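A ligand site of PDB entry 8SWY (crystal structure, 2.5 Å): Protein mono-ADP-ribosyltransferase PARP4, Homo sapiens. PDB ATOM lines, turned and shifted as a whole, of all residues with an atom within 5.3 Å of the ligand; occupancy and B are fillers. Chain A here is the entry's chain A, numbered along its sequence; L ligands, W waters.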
ATOM      1  N   LEU A 123     -12.097  -1.326  -4.458  1.00  0.00           N
ATOM      2  CA  LEU A 123     -13.406  -1.283  -5.101  1.00  0.00           C
ATOM      3  C   LEU A 123     -14.325  -0.281  -4.414  1.00  0.00           C
ATOM      4  O   LEU A 123     -14.366  -0.189  -3.183  1.00  0.00           O
ATOM      5  CB  LEU A 123     -14.034  -2.669  -5.053  1.00  0.00           C
ATOM      6  CG  LEU A 123     -13.175  -3.783  -5.655  1.00  0.00           C
ATOM      7  CD1 LEU A 123     -13.889  -5.116  -5.537  1.00  0.00           C
ATOM      8  CD2 LEU A 123     -12.789  -3.475  -7.140  1.00  0.00           C
ATOM      9  N   HIS A 124     -15.092   0.460  -5.201  1.00  0.00           N
ATOM     10  CA  HIS A 124     -16.101   1.380  -4.688  1.00  0.00           C
ATOM     11  C   HIS A 124     -17.359   1.157  -5.501  1.00  0.00           C
ATOM     12  O   HIS A 124     -17.348   1.326  -6.719  1.00  0.00           O
ATOM     13  CB  HIS A 124     -15.646   2.853  -4.802  1.00  0.00           C
ATOM     14  CG  HIS A 124     -16.639   3.851  -4.319  1.00  0.00           C
ATOM     15  ND1 HIS A 124     -16.818   4.165  -2.992  1.00  0.00           N
ATOM     16  CD2 HIS A 124     -17.524   4.629  -5.006  1.00  0.00           C
ATOM     17  CE1 HIS A 124     -17.763   5.074  -2.876  1.00  0.00           C
ATOM     18  NE2 HIS A 124     -18.205   5.378  -4.077  1.00  0.00           N
ATOM     19  N   GLY A 125     -18.428   0.757  -4.842  1.00  0.00           N
ATOM     20  CA  GLY A 125     -19.690   0.580  -5.511  1.00  0.00           C
ATOM     21  C   GLY A 125     -20.517   1.852  -5.429  1.00  0.00           C
ATOM     22  O   GLY A 125     -20.402   2.618  -4.470  1.00  0.00           O
ATOM     23  N   SER A 126     -21.317   2.084  -6.474  1.00  0.00           N
ATOM     24  CA  SER A 126     -22.231   3.231  -6.557  1.00  0.00           C
ATOM     25  C   SER A 126     -23.391   2.890  -7.476  1.00  0.00           C
ATOM     26  O   SER A 126     -23.203   2.167  -8.466  1.00  0.00           O
ATOM     27  CB  SER A 126     -21.549   4.504  -7.069  1.00  0.00           C
ATOM     28  OG  SER A 126     -22.295   5.651  -6.658  1.00  0.00           O
ATOM     29  N   PRO A 127     -24.590   3.376  -7.171  1.00  0.00           N
ATOM     30  CA  PRO A 127     -25.698   3.272  -8.142  1.00  0.00           C
ATOM     31  C   PRO A 127     -25.340   3.928  -9.465  1.00  0.00           C
ATOM     32  O   PRO A 127     -24.552   4.874  -9.516  1.00  0.00           O
ATOM     33  CB  PRO A 127     -26.853   4.013  -7.449  1.00  0.00           C
ATOM     34  CG  PRO A 127     -26.212   4.780  -6.328  1.00  0.00           C
ATOM     35  CD  PRO A 127     -25.006   3.999  -5.913  1.00  0.00           C
ATOM     36  N   ASN A 130     -25.219   7.777 -10.364  1.00  0.00           N
ATOM     37  CA  ASN A 130     -24.160   8.651  -9.883  1.00  0.00           C
ATOM     38  C   ASN A 130     -22.959   8.706 -10.799  1.00  0.00           C
ATOM     39  O   ASN A 130     -22.113   9.586 -10.623  1.00  0.00           O
ATOM     40  CB  ASN A 130     -23.699   8.217  -8.490  1.00  0.00           C
ATOM     41  CG  ASN A 130     -24.755   8.442  -7.436  1.00  0.00           C
ATOM     42  OD1 ASN A 130     -25.650   9.244  -7.611  1.00  0.00           O
ATOM     43  ND2 ASN A 130     -24.642   7.728  -6.326  1.00  0.00           N
ATOM     44  N   GLY A 133     -21.773  11.821 -12.710  1.00  0.00           N
ATOM     45  CA  GLY A 133     -21.262  12.821 -11.792  1.00  0.00           C
ATOM     46  C   GLY A 133     -19.940  12.441 -11.197  1.00  0.00           C
ATOM     47  O   GLY A 133     -19.095  13.310 -10.936  1.00  0.00           O
ATOM     48  N   ILE A 134     -19.742  11.148 -10.953  1.00  0.00           N
ATOM     49  CA  ILE A 134     -18.479  10.640 -10.427  1.00  0.00           C
ATOM     50  C   ILE A 134     -17.360  10.812 -11.436  1.00  0.00           C
ATOM     51  O   ILE A 134     -16.226  11.143 -11.076  1.00  0.00           O
ATOM     52  CB  ILE A 134     -18.649   9.170 -10.013  1.00  0.00           C
ATOM     53  CG1 ILE A 134     -19.488   9.069  -8.730  1.00  0.00           C
ATOM     54  CG2 ILE A 134     -17.285   8.550  -9.851  1.00  0.00           C
ATOM     55  CD1 ILE A 134     -19.937   7.672  -8.418  1.00  0.00           C
ATOM     56  N   ARG A 137     -16.523  14.649 -11.678  1.00  0.00           N
ATOM     57  CA  ARG A 137     -16.069  15.360 -10.478  1.00  0.00           C
ATOM     58  C   ARG A 137     -15.126  14.565  -9.599  1.00  0.00           C
ATOM     59  O   ARG A 137     -14.462  15.168  -8.744  1.00  0.00           O
ATOM     60  CB  ARG A 137     -17.265  15.794  -9.612  1.00  0.00           C
ATOM     61  CG  ARG A 137     -18.190  16.812 -10.197  1.00  0.00           C
ATOM     62  CD  ARG A 137     -17.481  18.158 -10.364  1.00  0.00           C
ATOM     63  NE  ARG A 137     -16.995  18.685  -9.094  1.00  0.00           N
ATOM     64  CZ  ARG A 137     -17.723  19.338  -8.192  1.00  0.00           C
ATOM     65  NH1 ARG A 137     -19.013  19.589  -8.377  1.00  0.00           N
ATOM     66  NH2 ARG A 137     -17.156  19.748  -7.059  1.00  0.00           N
ATOM     67  N   GLY A 138     -14.990  13.264  -9.795  1.00  0.00           N
ATOM     68  CA  GLY A 138     -14.303  12.414  -8.854  1.00  0.00           C
ATOM     69  C   GLY A 138     -15.217  12.040  -7.698  1.00  0.00           C
ATOM     70  O   GLY A 138     -16.271  12.629  -7.491  1.00  0.00           O
ATOM     71  N   LEU A 139     -14.811  11.022  -6.944  1.00  0.00           N
ATOM     72  CA  LEU A 139     -15.463  10.786  -5.659  1.00  0.00           C
ATOM     73  C   LEU A 139     -15.298  11.986  -4.738  1.00  0.00           C
ATOM     74  O   LEU A 139     -14.180  12.489  -4.548  1.00  0.00           O
ATOM     75  CB  LEU A 139     -14.897   9.528  -5.006  1.00  0.00           C
ATOM     76  CG  LEU A 139     -15.189   8.247  -5.817  1.00  0.00           C
ATOM     77  CD1 LEU A 139     -14.408   7.032  -5.292  1.00  0.00           C
ATOM     78  CD2 LEU A 139     -16.685   7.949  -5.848  1.00  0.00           C
ATOM     79  N   LEU A 140     -16.381  12.447  -4.135  1.00  0.00           N
ATOM     80  CA  LEU A 140     -16.348  13.625  -3.276  1.00  0.00           C
ATOM     81  C   LEU A 140     -16.627  13.237  -1.847  1.00  0.00           C
ATOM     82  O   LEU A 140     -17.262  12.217  -1.581  1.00  0.00           O
ATOM     83  CB  LEU A 140     -17.360  14.689  -3.699  1.00  0.00           C
ATOM     84  CG  LEU A 140     -17.284  15.190  -5.142  1.00  0.00           C
ATOM     85  CD1 LEU A 140     -18.570  15.881  -5.493  1.00  0.00           C
ATOM     86  CD2 LEU A 140     -16.074  16.133  -5.316  1.00  0.00           C
ATOM     87  N   PRO A 142     -18.626  13.526   1.602  1.00  0.00           N
ATOM     88  CA  PRO A 142     -19.995  13.934   1.955  1.00  0.00           C
ATOM     89  C   PRO A 142     -19.975  15.210   2.762  1.00  0.00           C
ATOM     90  O   PRO A 142     -18.956  15.568   3.358  1.00  0.00           O
ATOM     91  CB  PRO A 142     -20.507  12.760   2.796  1.00  0.00           C
ATOM     92  CG  PRO A 142     -19.280  11.976   3.206  1.00  0.00           C
ATOM     93  CD  PRO A 142     -18.084  12.493   2.486  1.00  0.00           C
ATOM     94  N   VAL A 155     -24.588   9.557   7.651  1.00  0.00           N
ATOM     95  CA  VAL A 155     -23.190   9.281   7.967  1.00  0.00           C
ATOM     96  C   VAL A 155     -22.896   7.788   7.798  1.00  0.00           C
ATOM     97  O   VAL A 155     -23.642   6.938   8.307  1.00  0.00           O
ATOM     98  CB  VAL A 155     -22.827   9.689   9.414  1.00  0.00           C
ATOM     99  CG1 VAL A 155     -21.337   9.633   9.623  1.00  0.00           C
ATOM    100  CG2 VAL A 155     -23.345  11.076   9.744  1.00  0.00           C
ATOM    101  N   GLY A 156     -21.820   7.465   7.064  1.00  0.00           N
ATOM    102  CA  GLY A 156     -21.295   6.117   7.101  1.00  0.00           C
ATOM    103  C   GLY A 156     -20.849   5.724   8.498  1.00  0.00           C
ATOM    104  O   GLY A 156     -20.640   6.560   9.386  1.00  0.00           O
ATOM    105  N   ASN A 157     -20.708   4.426   8.721  1.00  0.00           N
ATOM    106  CA  ASN A 157     -20.390   4.026  10.095  1.00  0.00           C
ATOM    107  C   ASN A 157     -18.954   4.334  10.487  1.00  0.00           C
ATOM    108  O   ASN A 157     -18.535   3.982  11.593  1.00  0.00           O
ATOM    109  CB  ASN A 157     -20.750   2.549  10.334  1.00  0.00           C
ATOM    110  CG  ASN A 157     -20.159   1.622   9.304  1.00  0.00           C
ATOM    111  OD1 ASN A 157     -18.978   1.714   8.966  1.00  0.00           O
ATOM    112  ND2 ASN A 157     -20.985   0.712   8.773  1.00  0.00           N
ATOM    113  N   LEU A 158     -18.173   5.003   9.640  1.00  0.00           N
ATOM    114  CA  LEU A 158     -16.871   5.524  10.033  1.00  0.00           C
ATOM    115  C   LEU A 158     -16.770   7.007   9.672  1.00  0.00           C
ATOM    116  O   LEU A 158     -15.700   7.512   9.302  1.00  0.00           O
ATOM    117  CB  LEU A 158     -15.736   4.714   9.400  1.00  0.00           C
ATOM    118  CG  LEU A 158     -15.435   3.334  10.011  1.00  0.00           C
ATOM    119  CD1 LEU A 158     -14.580   2.480   9.072  1.00  0.00           C
ATOM    120  CD2 LEU A 158     -14.730   3.482  11.309  1.00  0.00           C
ATOM    121  N   GLY A 161     -16.348  10.217   5.327  1.00  0.00           N
ATOM    122  CA  GLY A 161     -15.247   9.980   4.406  1.00  0.00           C
ATOM    123  C   GLY A 161     -15.653   9.317   3.104  1.00  0.00           C
ATOM    124  O   GLY A 161     -16.839   9.176   2.830  1.00  0.00           O
ATOM    125  N   TYR A 163     -15.567   5.807   1.019  1.00  0.00           N
ATOM    126  CA  TYR A 163     -15.575   4.405   1.454  1.00  0.00           C
ATOM    127  C   TYR A 163     -15.201   3.442   0.328  1.00  0.00           C
ATOM    128  O   TYR A 163     -15.773   3.508  -0.772  1.00  0.00           O
ATOM    129  CB  TYR A 163     -16.943   4.012   1.992  1.00  0.00           C
ATOM    130  CG  TYR A 163     -17.273   4.577   3.338  1.00  0.00           C
ATOM    131  CD1 TYR A 163     -17.630   5.915   3.485  1.00  0.00           C
ATOM    132  CD2 TYR A 163     -17.234   3.782   4.457  1.00  0.00           C
ATOM    133  CE1 TYR A 163     -17.930   6.434   4.720  1.00  0.00           C
ATOM    134  CE2 TYR A 163     -17.533   4.279   5.696  1.00  0.00           C
ATOM    135  CZ  TYR A 163     -17.886   5.612   5.821  1.00  0.00           C
ATOM    136  OH  TYR A 163     -18.183   6.111   7.046  1.00  0.00           O
ATOM    137  N   PHE A 164     -14.318   2.492   0.638  1.00  0.00           N
ATOM    138  CA  PHE A 164     -13.910   1.467  -0.306  1.00  0.00           C
ATOM    139  C   PHE A 164     -13.956   0.106   0.382  1.00  0.00           C
ATOM    140  O   PHE A 164     -14.045   0.007   1.595  1.00  0.00           O
ATOM    141  CB  PHE A 164     -12.490   1.718  -0.816  1.00  0.00           C
ATOM    142  CG  PHE A 164     -12.311   3.051  -1.492  1.00  0.00           C
ATOM    143  CD1 PHE A 164     -11.991   4.173  -0.759  1.00  0.00           C
ATOM    144  CD2 PHE A 164     -12.466   3.170  -2.874  1.00  0.00           C
ATOM    145  CE1 PHE A 164     -11.831   5.425  -1.378  1.00  0.00           C
ATOM    146  CE2 PHE A 164     -12.304   4.407  -3.495  1.00  0.00           C
ATOM    147  CZ  PHE A 164     -11.985   5.528  -2.747  1.00  0.00           C
ATOM    148  N   SER A 165     -13.908  -0.946  -0.427  1.00  0.00           N
ATOM    149  CA  SER A 165     -13.726  -2.303   0.065  1.00  0.00           C
ATOM    150  C   SER A 165     -12.676  -3.018  -0.773  1.00  0.00           C
ATOM    151  O   SER A 165     -12.400  -2.659  -1.926  1.00  0.00           O
ATOM    152  CB  SER A 165     -15.022  -3.129   0.031  1.00  0.00           C
ATOM    153  OG  SER A 165     -14.781  -4.456   0.513  1.00  0.00           O
ATOM    154  N   THR A 170     -18.711  -7.052  -1.022  1.00  0.00           N
ATOM    155  CA  THR A 170     -19.173  -5.823  -0.372  1.00  0.00           C
ATOM    156  C   THR A 170     -19.702  -4.827  -1.403  1.00  0.00           C
ATOM    157  O   THR A 170     -20.781  -4.251  -1.229  1.00  0.00           O
ATOM    158  CB  THR A 170     -18.024  -5.223   0.425  1.00  0.00           C
ATOM    159  OG1 THR A 170     -17.631  -6.162   1.435  1.00  0.00           O
ATOM    160  CG2 THR A 170     -18.403  -3.863   1.033  1.00  0.00           C
ATOM    161  N   SER A 171     -18.930  -4.630  -2.493  1.00  0.00           N
ATOM    162  CA  SER A 171     -19.291  -3.624  -3.496  1.00  0.00           C
ATOM    163  C   SER A 171     -20.664  -3.897  -4.091  1.00  0.00           C
ATOM    164  O   SER A 171     -21.348  -2.956  -4.516  1.00  0.00           O
ATOM    165  CB  SER A 171     -18.261  -3.613  -4.618  1.00  0.00           C
ATOM    166  OG  SER A 171     -16.971  -3.254  -4.157  1.00  0.00           O
ATOM    167  N   TYR A 174     -23.641  -1.861  -2.947  1.00  0.00           N
ATOM    168  CA  TYR A 174     -23.763  -0.454  -3.324  1.00  0.00           C
ATOM    169  C   TYR A 174     -23.843  -0.224  -4.825  1.00  0.00           C
ATOM    170  O   TYR A 174     -24.231   0.883  -5.248  1.00  0.00           O
ATOM    171  CB  TYR A 174     -22.604   0.372  -2.709  1.00  0.00           C
ATOM    172  CG  TYR A 174     -22.489  -0.034  -1.259  1.00  0.00           C
ATOM    173  CD1 TYR A 174     -23.500   0.339  -0.358  1.00  0.00           C
ATOM    174  CD2 TYR A 174     -21.467  -0.850  -0.805  1.00  0.00           C
ATOM    175  CE1 TYR A 174     -23.467  -0.065   0.946  1.00  0.00           C
ATOM    176  CE2 TYR A 174     -21.415  -1.254   0.516  1.00  0.00           C
ATOM    177  CZ  TYR A 174     -22.427  -0.857   1.398  1.00  0.00           C
ATOM    178  OH  TYR A 174     -22.419  -1.237   2.717  1.00  0.00           O
ATOM    179  N   ASP A 232     -15.170  -5.484   5.288  1.00  0.00           N
ATOM    180  CA  ASP A 232     -13.985  -4.677   5.414  1.00  0.00           C
ATOM    181  C   ASP A 232     -14.228  -3.351   4.716  1.00  0.00           C
ATOM    182  O   ASP A 232     -14.645  -3.321   3.550  1.00  0.00           O
ATOM    183  CB  ASP A 232     -12.767  -5.390   4.841  1.00  0.00           C
ATOM    184  CG  ASP A 232     -12.238  -6.452   5.769  1.00  0.00           C
ATOM    185  OD1 ASP A 232     -11.814  -6.123   6.895  1.00  0.00           O
ATOM    186  OD2 ASP A 232     -12.242  -7.638   5.380  1.00  0.00           O
ATOM    187  N   GLU A 233     -13.973  -2.262   5.423  1.00  0.00           N
ATOM    188  CA  GLU A 233     -14.198  -0.934   4.893  1.00  0.00           C
ATOM    189  C   GLU A 233     -12.882  -0.187   5.004  1.00  0.00           C
ATOM    190  O   GLU A 233     -12.222  -0.241   6.037  1.00  0.00           O
ATOM    191  CB  GLU A 233     -15.282  -0.209   5.677  1.00  0.00           C
ATOM    192  CG  GLU A 233     -16.516  -1.022   5.926  1.00  0.00           C
ATOM    193  CD  GLU A 233     -17.616  -0.214   6.606  1.00  0.00           C
ATOM    194  OE1 GLU A 233     -17.442   1.016   6.820  1.00  0.00           O
ATOM    195  OE2 GLU A 233     -18.685  -0.793   6.879  1.00  0.00           O
HETATM  196  P1  LIG L   1     -22.345   7.703   1.635  1.00  0.00           P
HETATM  197  O1  LIG L   1     -23.401   7.164   2.541  1.00  0.00           O
HETATM  198  O2  LIG L   1     -21.486   8.868   2.171  1.00  0.00           O
HETATM  199  O3  LIG L   1     -22.937   8.091   0.198  1.00  0.00           O
HETATM  200  C1  LIG L   1     -22.219   8.947  -0.715  1.00  0.00           C
HETATM  201  C2  LIG L   1     -22.468   8.469  -2.123  1.00  0.00           C
HETATM  202  O4  LIG L   1     -22.124   9.525  -3.051  1.00  0.00           O
HETATM  203  C3  LIG L   1     -21.698   7.212  -2.548  1.00  0.00           C
HETATM  204  O5  LIG L   1     -22.566   6.158  -2.954  1.00  0.00           O
HETATM  205  C4  LIG L   1     -20.805   7.692  -3.711  1.00  0.00           C
HETATM  206  O6  LIG L   1     -20.846   6.709  -4.745  1.00  0.00           O
HETATM  207  C5  LIG L   1     -21.508   8.960  -4.184  1.00  0.00           C
HETATM  208  N1  LIG L   1     -20.626   9.974  -4.775  1.00  0.00           N
HETATM  209  C6  LIG L   1     -19.375  10.353  -4.336  1.00  0.00           C
HETATM  210  N2  LIG L   1     -18.837  11.312  -5.047  1.00  0.00           N
HETATM  211  C7  LIG L   1     -19.781  11.581  -6.024  1.00  0.00           C
HETATM  212  C8  LIG L   1     -19.818  12.494  -7.104  1.00  0.00           C
HETATM  213  N3  LIG L   1     -18.824  13.332  -7.398  1.00  0.00           N
HETATM  214  N4  LIG L   1     -20.935  12.513  -7.879  1.00  0.00           N
HETATM  215  C9  LIG L   1     -21.923  11.657  -7.608  1.00  0.00           C
HETATM  216  N5  LIG L   1     -22.009  10.762  -6.619  1.00  0.00           N
HETATM  217  C10 LIG L   1     -20.903  10.771  -5.856  1.00  0.00           C
HETATM  218  O7  LIG L   1     -21.338   6.526   1.264  1.00  0.00           O
HETATM  219  P2  LIG L   1     -21.443   5.072   0.637  1.00  0.00           P
HETATM  220  O8  LIG L   1     -20.061   4.708   0.076  1.00  0.00           O
HETATM  221  O9  LIG L   1     -22.532   5.010  -0.362  1.00  0.00           O
HETATM  222  O10 LIG L   1     -21.829   4.198   1.889  1.00  0.00           O
HETATM  223  C11 LIG L   1     -21.110   4.283   3.136  1.00  0.00           C
HETATM  224  C12 LIG L   1     -21.474   3.044   3.905  1.00  0.00           C
HETATM  225  O11 LIG L   1     -21.497   1.909   3.003  1.00  0.00           O
HETATM  226  C13 LIG L   1     -20.546   2.691   5.070  1.00  0.00           C
HETATM  227  O12 LIG L   1     -21.176   2.973   6.311  1.00  0.00           O
HETATM  228  C14 LIG L   1     -20.333   1.169   4.930  1.00  0.00           C
HETATM  229  O13 LIG L   1     -21.281   0.429   5.719  1.00  0.00           O
HETATM  230  C15 LIG L   1     -20.597   0.921   3.446  1.00  0.00           C
HETATM  231  N6  LIG L   1     -19.391   0.931   2.603  1.00  0.00           N
HETATM  232  C16 LIG L   1     -19.443   1.449   1.349  1.00  0.00           C
HETATM  233  C17 LIG L   1     -18.659   0.912   0.383  1.00  0.00           C
HETATM  234  C18 LIG L   1     -18.829   1.428  -0.971  1.00  0.00           C
HETATM  235  O14 LIG L   1     -18.503   0.759  -1.973  1.00  0.00           O
HETATM  236  N7  LIG L   1     -19.357   2.645  -1.114  1.00  0.00           N
HETATM  237  C19 LIG L   1     -17.546  -0.034   0.713  1.00  0.00           C
HETATM  238  C20 LIG L   1     -17.472  -0.262   2.185  1.00  0.00           C
HETATM  239  C21 LIG L   1     -18.234   0.369   3.058  1.00  0.00           C
HETATM  240  O   HOH W   1     -16.766  -1.144  -2.516  1.00  0.00           O
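The side-chain hydroxyl (OG) of Ser 126 sits at hydrogen-bond distance from an oxygen (O6) of the ligand, at 2.6 Å. The backbone carbonyl oxygen (O) of Gly 138 is in hydrogen-bond range of a nitrogen (N3) of the ligand, at 2.6 Å. The backbone NH (N) of Asn 157 sits at hydrogen-bond distance from an oxygen (O12) of the ligand, 2.9 Å away. The side-chain amide nitrogen (ND2) of Asn 157 lies within hydrogen-bond range of an oxygen (O13) of the ligand. N2 of the ligand sits at hydrogen-bond distance from N of Leu 140, 2.9 Å away. N of Gly 125 is in hydrogen-bond range of O14 of the ligand, at 2.9 Å. An oxygen (O11) of the ligand sits close to the side-chain hydroxyl of Tyr 174, at 3.3 Å. NE2 of His 124 lies within hydrogen-bond range of O6 of the ligand (3.0 Å). An oxygen (O13) of the ligand is in hydrogen-bond range of the side-chain carboxylate of Glu 233, 3.1 Å away.
N of Ser 126 lies close to O of Tyr 174 (3.4 Å). The side-chain hydroxyl (OG) of Ser 126 sits at hydrogen-bond distance from the side-chain amide nitrogen (ND2) of Asn 130, at 3.2 Å. The side-chain amide oxygen (OD1) of Asn 157 sits close to the side-chain carboxylate (OE1) of Glu 233, 2.7 Å away. The backbone NH (N) of Asn 157 lies within hydrogen-bond range of the side-chain hydroxyl (OH) of Tyr 163, at 3.5 Å. A ring nitrogen (ND1) of His 124 is in hydrogen-bond range of the backbone carbonyl oxygen (O) of Tyr 163, 2.5 Å away. The backbone carbonyl oxygen (O) of Gly 156 lies close to the side-chain hydroxyl (OH) of Tyr 163. The side-chain hydroxyl (OG) of Ser 165 is in hydrogen-bond range of the backbone carbonyl oxygen (O) of Asp 232, 3.2 Å away. O of Ser 165 is in hydrogen-bond range of N of Leu 123 (2.9 Å).
Asn 130 touches the ligand. Gly 133 touches the ligand. N of Ile 134 touches N4 of the ligand, at 3.6 Å. CB of Arg 137 touches N3 of the ligand, 3.7 Å away. CA of Leu 139 touches N2 of the ligand, 3.5 Å away. CG of Pro 142 touches O2 of the ligand, 3.9 Å away. Gly 156 touches the ligand (CA to O12, 3.2 Å). Tyr 163 touches the ligand (CE2 to C13, 3.5 Å). O of Phe 164 touches C20 of the ligand, at 3.5 Å. Ser 165 touches the ligand (N to C19, 3.9 Å). CG2 of Thr 170 touches C20 of the ligand, at 3.9 Å. Hydrophobic or aromatic side chains that line the ligand: His 124, Ile 134, Leu 139, Leu 140, Pro 142, Tyr 163 and Tyr 174. 19 residues have an atom within 4 Å of the ligand: His 124, Gly 125, Ser 126, Asn 130, Gly 133, Ile 134, Arg 137, Gly 138, Leu 139, Leu 140, Pro 142, Gly 156, Asn 157, Tyr 163, Phe 164, Ser 165, Thr 170, Tyr 174 and Glu 233. The nearest printed residue that does not touch the ligand is Asp 232 (4.4 Å).
Water W1 lies within hydrogen-bond range of O14 of the ligand (2.6 Å), O of Leu 123 (2.7 Å), OG of Ser 171 (2.7 Å) and N of Gly 125 (3.4 Å).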
